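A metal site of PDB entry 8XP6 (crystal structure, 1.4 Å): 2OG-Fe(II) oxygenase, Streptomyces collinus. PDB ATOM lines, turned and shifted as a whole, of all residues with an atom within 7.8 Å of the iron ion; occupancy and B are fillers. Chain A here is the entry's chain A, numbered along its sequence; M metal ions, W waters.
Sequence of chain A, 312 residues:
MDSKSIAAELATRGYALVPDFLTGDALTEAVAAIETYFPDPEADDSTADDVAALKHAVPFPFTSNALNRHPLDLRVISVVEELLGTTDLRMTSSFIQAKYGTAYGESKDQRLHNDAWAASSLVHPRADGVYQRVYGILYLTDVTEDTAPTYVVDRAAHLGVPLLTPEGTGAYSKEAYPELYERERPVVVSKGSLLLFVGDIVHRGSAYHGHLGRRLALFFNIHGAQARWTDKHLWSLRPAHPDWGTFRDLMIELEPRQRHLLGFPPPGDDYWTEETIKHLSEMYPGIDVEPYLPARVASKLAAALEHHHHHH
Within 4 Å of the iron ion: His 113, Asp 115 and His 203. The nearest printed residue that does not touch the iron ion is Gln 110 (4.6 Å).
The iron ion is bound by OD2 of Asp 115 (2.0 Å), water W2 (2.0 Å), water W3 (2.1 Å), water W1 (2.2 Å), NE2 of His 203 (2.2 Å) and NE2 of His 113 (2.2 Å).
N of Asp 115 sits at hydrogen-bond distance from O of Gly 199 (2.7 Å). O of Arg 111 sits at hydrogen-bond distance from ND1 of His 113 (2.9 Å). A ring nitrogen (ND1) of His 203 sits at hydrogen-bond distance from the backbone carbonyl oxygen (O) of Ile 201 (3.0 Å).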
ATOM      1  N   GLN A 110      -9.853 -36.770 -14.616  1.00  0.00           N
ATOM      2  CA  GLN A 110      -8.841 -36.029 -15.354  1.00  0.00           C
ATOM      3  C   GLN A 110      -7.462 -36.440 -14.843  1.00  0.00           C
ATOM      4  O   GLN A 110      -7.304 -36.958 -13.740  1.00  0.00           O
ATOM      5  CB  GLN A 110      -9.000 -34.515 -15.137  1.00  0.00           C
ATOM      6  CG  GLN A 110     -10.283 -33.913 -15.711  1.00  0.00           C
ATOM      7  CD  GLN A 110     -10.397 -32.420 -15.450  1.00  0.00           C
ATOM      8  OE1 GLN A 110      -9.876 -31.911 -14.458  1.00  0.00           O
ATOM      9  NE2 GLN A 110     -11.090 -31.720 -16.339  1.00  0.00           N
ATOM     10  N   ARG A 111      -6.449 -36.238 -15.696  1.00  0.00           N
ATOM     11  CA  ARG A 111      -5.081 -36.314 -15.198  1.00  0.00           C
ATOM     12  C   ARG A 111      -4.770 -35.077 -14.367  1.00  0.00           C
ATOM     13  O   ARG A 111      -5.350 -34.006 -14.564  1.00  0.00           O
ATOM     14  CB  ARG A 111      -4.101 -36.386 -16.369  1.00  0.00           C
ATOM     15  CG  ARG A 111      -4.176 -37.706 -17.141  1.00  0.00           C
ATOM     16  CD  ARG A 111      -3.031 -37.860 -18.111  1.00  0.00           C
ATOM     17  NE  ARG A 111      -3.034 -36.790 -19.097  1.00  0.00           N
ATOM     18  CZ  ARG A 111      -1.995 -36.488 -19.866  1.00  0.00           C
ATOM     19  NH1 ARG A 111      -0.866 -37.158 -19.750  1.00  0.00           N
ATOM     20  NH2 ARG A 111      -2.091 -35.492 -20.740  1.00  0.00           N
ATOM     21  N   LEU A 112      -3.856 -35.229 -13.417  1.00  0.00           N
ATOM     22  CA  LEU A 112      -3.338 -34.066 -12.718  1.00  0.00           C
ATOM     23  C   LEU A 112      -2.720 -33.099 -13.724  1.00  0.00           C
ATOM     24  O   LEU A 112      -2.055 -33.497 -14.679  1.00  0.00           O
ATOM     25  CB  LEU A 112      -2.290 -34.492 -11.666  1.00  0.00           C
ATOM     26  CG  LEU A 112      -2.825 -35.136 -10.387  1.00  0.00           C
ATOM     27  CD1 LEU A 112      -1.686 -35.603  -9.495  1.00  0.00           C
ATOM     28  CD2 LEU A 112      -3.731 -34.193  -9.615  1.00  0.00           C
ATOM     29  N   HIS A 113      -2.952 -31.814 -13.503  1.00  0.00           N
ATOM     30  CA  HIS A 113      -2.480 -30.792 -14.420  1.00  0.00           C
ATOM     31  C   HIS A 113      -2.419 -29.460 -13.687  1.00  0.00           C
ATOM     32  O   HIS A 113      -2.963 -29.292 -12.591  1.00  0.00           O
ATOM     33  CB  HIS A 113      -3.406 -30.696 -15.642  1.00  0.00           C
ATOM     34  CG  HIS A 113      -4.799 -30.271 -15.303  1.00  0.00           C
ATOM     35  ND1 HIS A 113      -5.756 -31.158 -14.842  1.00  0.00           N
ATOM     36  CD2 HIS A 113      -5.397 -29.050 -15.319  1.00  0.00           C
ATOM     37  CE1 HIS A 113      -6.877 -30.499 -14.605  1.00  0.00           C
ATOM     38  NE2 HIS A 113      -6.688 -29.220 -14.892  1.00  0.00           N
ATOM     39  N   ASN A 114      -1.738 -28.500 -14.307  1.00  0.00           N
ATOM     40  CA  ASN A 114      -1.851 -27.113 -13.906  1.00  0.00           C
ATOM     41  C   ASN A 114      -2.712 -26.351 -14.908  1.00  0.00           C
ATOM     42  O   ASN A 114      -2.860 -26.739 -16.061  1.00  0.00           O
ATOM     43  CB  ASN A 114      -0.467 -26.448 -13.762  1.00  0.00           C
ATOM     44  CG  ASN A 114       0.186 -26.129 -15.091  1.00  0.00           C
ATOM     45  OD1 ASN A 114      -0.244 -25.211 -15.786  1.00  0.00           O
ATOM     46  ND2 ASN A 114       1.218 -26.878 -15.460  1.00  0.00           N
ATOM     47  N   ASP A 115      -3.302 -25.251 -14.422  1.00  0.00           N
ATOM     48  CA  ASP A 115      -4.023 -24.312 -15.277  1.00  0.00           C
ATOM     49  C   ASP A 115      -3.344 -22.951 -15.224  1.00  0.00           C
ATOM     50  O   ASP A 115      -3.984 -21.915 -15.056  1.00  0.00           O
ATOM     51  CB  ASP A 115      -5.501 -24.225 -14.892  1.00  0.00           C
ATOM     52  CG  ASP A 115      -6.300 -25.378 -15.431  1.00  0.00           C
ATOM     53  OD1 ASP A 115      -6.339 -25.564 -16.666  1.00  0.00           O
ATOM     54  OD2 ASP A 115      -6.876 -26.125 -14.638  1.00  0.00           O
ATOM     55  N   ALA A 116      -2.014 -22.946 -15.363  1.00  0.00           N
ATOM     56  CA  ALA A 116      -1.248 -21.713 -15.342  1.00  0.00           C
ATOM     57  C   ALA A 116      -1.258 -21.005 -16.683  1.00  0.00           C
ATOM     58  O   ALA A 116      -0.882 -19.829 -16.723  1.00  0.00           O
ATOM     59  CB  ALA A 116       0.202 -22.034 -14.979  1.00  0.00           C
ATOM     60  N   TYR A 135      -8.733 -19.455  -9.751  1.00  0.00           N
ATOM     61  CA  TYR A 135      -9.894 -20.282 -10.053  1.00  0.00           C
ATOM     62  C   TYR A 135     -10.801 -20.396  -8.841  1.00  0.00           C
ATOM     63  O   TYR A 135     -10.350 -20.443  -7.688  1.00  0.00           O
ATOM     64  CB  TYR A 135      -9.404 -21.681 -10.444  1.00  0.00           C
ATOM     65  CG  TYR A 135      -8.893 -21.755 -11.846  1.00  0.00           C
ATOM     66  CD1 TYR A 135      -9.621 -22.397 -12.836  1.00  0.00           C
ATOM     67  CD2 TYR A 135      -7.681 -21.154 -12.202  1.00  0.00           C
ATOM     68  CE1 TYR A 135      -9.172 -22.432 -14.145  1.00  0.00           C
ATOM     69  CE2 TYR A 135      -7.233 -21.182 -13.531  1.00  0.00           C
ATOM     70  CZ  TYR A 135      -7.986 -21.826 -14.477  1.00  0.00           C
ATOM     71  OH  TYR A 135      -7.541 -21.852 -15.772  1.00  0.00           O
ATOM     72  N   ILE A 137     -14.389 -22.705  -7.571  1.00  0.00           N
ATOM     73  CA  ILE A 137     -15.427 -23.706  -7.751  1.00  0.00           C
ATOM     74  C   ILE A 137     -16.399 -23.524  -6.589  1.00  0.00           C
ATOM     75  O   ILE A 137     -16.037 -23.768  -5.430  1.00  0.00           O
ATOM     76  CB  ILE A 137     -14.900 -25.142  -7.802  1.00  0.00           C
ATOM     77  CG1 ILE A 137     -13.785 -25.298  -8.847  1.00  0.00           C
ATOM     78  CG2 ILE A 137     -16.063 -26.104  -8.104  1.00  0.00           C
ATOM     79  CD1 ILE A 137     -13.152 -26.701  -8.864  1.00  0.00           C
ATOM     80  N   THR A 150     -13.011 -32.410  -6.259  1.00  0.00           N
ATOM     81  CA  THR A 150     -11.773 -31.853  -6.795  1.00  0.00           C
ATOM     82  C   THR A 150     -10.602 -32.435  -6.005  1.00  0.00           C
ATOM     83  O   THR A 150     -10.667 -32.554  -4.777  1.00  0.00           O
ATOM     84  CB  THR A 150     -11.781 -30.343  -6.615  1.00  0.00           C
ATOM     85  OG1 THR A 150     -13.000 -29.783  -7.121  1.00  0.00           O
ATOM     86  CG2 THR A 150     -10.609 -29.711  -7.358  1.00  0.00           C
ATOM     87  N   PHE A 197      -8.369 -21.506  -5.898  1.00  0.00           N
ATOM     88  CA  PHE A 197      -7.026 -22.044  -6.099  1.00  0.00           C
ATOM     89  C   PHE A 197      -6.282 -21.234  -7.151  1.00  0.00           C
ATOM     90  O   PHE A 197      -6.894 -20.627  -8.026  1.00  0.00           O
ATOM     91  CB  PHE A 197      -6.989 -23.546  -6.374  1.00  0.00           C
ATOM     92  CG  PHE A 197      -7.714 -24.024  -7.620  1.00  0.00           C
ATOM     93  CD1 PHE A 197      -7.072 -24.103  -8.843  1.00  0.00           C
ATOM     94  CD2 PHE A 197      -9.036 -24.473  -7.535  1.00  0.00           C
ATOM     95  CE1 PHE A 197      -7.736 -24.605  -9.970  1.00  0.00           C
ATOM     96  CE2 PHE A 197      -9.690 -24.963  -8.646  1.00  0.00           C
ATOM     97  CZ  PHE A 197      -9.051 -25.025  -9.873  1.00  0.00           C
ATOM     98  N   GLY A 199      -3.932 -20.875 -10.439  1.00  0.00           N
ATOM     99  CA  GLY A 199      -3.915 -21.693 -11.643  1.00  0.00           C
ATOM    100  C   GLY A 199      -2.719 -22.613 -11.718  1.00  0.00           C
ATOM    101  O   GLY A 199      -2.800 -23.686 -12.322  1.00  0.00           O
ATOM    102  N   ILE A 201      -1.496 -24.390  -9.399  1.00  0.00           N
ATOM    103  CA  ILE A 201      -1.625 -25.581  -8.558  1.00  0.00           C
ATOM    104  C   ILE A 201      -1.785 -26.818  -9.435  1.00  0.00           C
ATOM    105  O   ILE A 201      -2.448 -26.779 -10.490  1.00  0.00           O
ATOM    106  CB  ILE A 201      -2.811 -25.441  -7.582  1.00  0.00           C
ATOM    107  CG1 ILE A 201      -2.601 -26.367  -6.378  1.00  0.00           C
ATOM    108  CG2 ILE A 201      -4.128 -25.781  -8.264  1.00  0.00           C
ATOM    109  CD1 ILE A 201      -3.741 -26.333  -5.361  1.00  0.00           C
ATOM    110  N   VAL A 202      -1.207 -27.919  -8.979  1.00  0.00           N
ATOM    111  CA  VAL A 202      -1.446 -29.234  -9.573  1.00  0.00           C
ATOM    112  C   VAL A 202      -2.745 -29.774  -8.985  1.00  0.00           C
ATOM    113  O   VAL A 202      -2.907 -29.857  -7.761  1.00  0.00           O
ATOM    114  CB  VAL A 202      -0.255 -30.150  -9.278  1.00  0.00           C
ATOM    115  CG1 VAL A 202      -0.502 -31.519  -9.883  1.00  0.00           C
ATOM    116  CG2 VAL A 202       1.025 -29.543  -9.849  1.00  0.00           C
ATOM    117  N   HIS A 203      -3.705 -30.100  -9.850  1.00  0.00           N
ATOM    118  CA  HIS A 203      -5.041 -30.475  -9.399  1.00  0.00           C
ATOM    119  C   HIS A 203      -5.715 -31.292 -10.504  1.00  0.00           C
ATOM    120  O   HIS A 203      -5.196 -31.410 -11.622  1.00  0.00           O
ATOM    121  CB  HIS A 203      -5.887 -29.226  -9.107  1.00  0.00           C
ATOM    122  CG  HIS A 203      -6.203 -28.447 -10.338  1.00  0.00           C
ATOM    123  ND1 HIS A 203      -5.264 -27.680 -11.000  1.00  0.00           N
ATOM    124  CD2 HIS A 203      -7.338 -28.389 -11.086  1.00  0.00           C
ATOM    125  CE1 HIS A 203      -5.815 -27.152 -12.082  1.00  0.00           C
ATOM    126  NE2 HIS A 203      -7.061 -27.580 -12.162  1.00  0.00           N
ATOM    127  N   ARG A 204      -6.890 -31.850 -10.186  1.00  0.00           N
ATOM    128  CA  ARG A 204      -7.688 -32.523 -11.208  1.00  0.00           C
ATOM    129  C   ARG A 204      -9.138 -32.656 -10.752  1.00  0.00           C
ATOM    130  O   ARG A 204      -9.416 -32.709  -9.547  1.00  0.00           O
ATOM    131  CB  ARG A 204      -7.127 -33.915 -11.511  1.00  0.00           C
ATOM    132  CG  ARG A 204      -7.220 -34.881 -10.329  1.00  0.00           C
ATOM    133  CD  ARG A 204      -6.642 -36.235 -10.692  1.00  0.00           C
ATOM    134  NE  ARG A 204      -6.783 -37.202  -9.618  1.00  0.00           N
ATOM    135  CZ  ARG A 204      -7.859 -37.957  -9.425  1.00  0.00           C
ATOM    136  NH1 ARG A 204      -8.917 -37.835 -10.234  1.00  0.00           N
ATOM    137  NH2 ARG A 204      -7.891 -38.813  -8.425  1.00  0.00           N
ATOM    138  N   GLY A 205     -10.038 -32.747 -11.738  1.00  0.00           N
ATOM    139  CA  GLY A 205     -11.352 -33.284 -11.473  1.00  0.00           C
ATOM    140  C   GLY A 205     -11.298 -34.788 -11.370  1.00  0.00           C
ATOM    141  O   GLY A 205     -10.340 -35.429 -11.803  1.00  0.00           O
ATOM    142  N   PHE A 219     -18.205 -22.750 -11.878  1.00  0.00           N
ATOM    143  CA  PHE A 219     -16.770 -22.560 -12.082  1.00  0.00           C
ATOM    144  C   PHE A 219     -16.508 -21.165 -12.614  1.00  0.00           C
ATOM    145  O   PHE A 219     -17.295 -20.625 -13.395  1.00  0.00           O
ATOM    146  CB  PHE A 219     -16.248 -23.536 -13.143  1.00  0.00           C
ATOM    147  CG  PHE A 219     -16.192 -24.964 -12.706  1.00  0.00           C
ATOM    148  CD1 PHE A 219     -14.974 -25.592 -12.553  1.00  0.00           C
ATOM    149  CD2 PHE A 219     -17.346 -25.689 -12.468  1.00  0.00           C
ATOM    150  CE1 PHE A 219     -14.883 -26.909 -12.168  1.00  0.00           C
ATOM    151  CE2 PHE A 219     -17.259 -27.019 -12.077  1.00  0.00           C
ATOM    152  CZ  PHE A 219     -16.027 -27.618 -11.923  1.00  0.00           C
HETATM  153 FE    FE M   1      -8.080 -27.658 -14.137  1.00  0.00          FE
HETATM  154  O   HOH W   1      -9.375 -25.987 -13.555  1.00  0.00           O
HETATM  155  O   HOH W   2      -9.028 -27.681 -15.927  1.00  0.00           O
HETATM  156  O   HOH W   3      -9.515 -29.076 -13.444  1.00  0.00           O
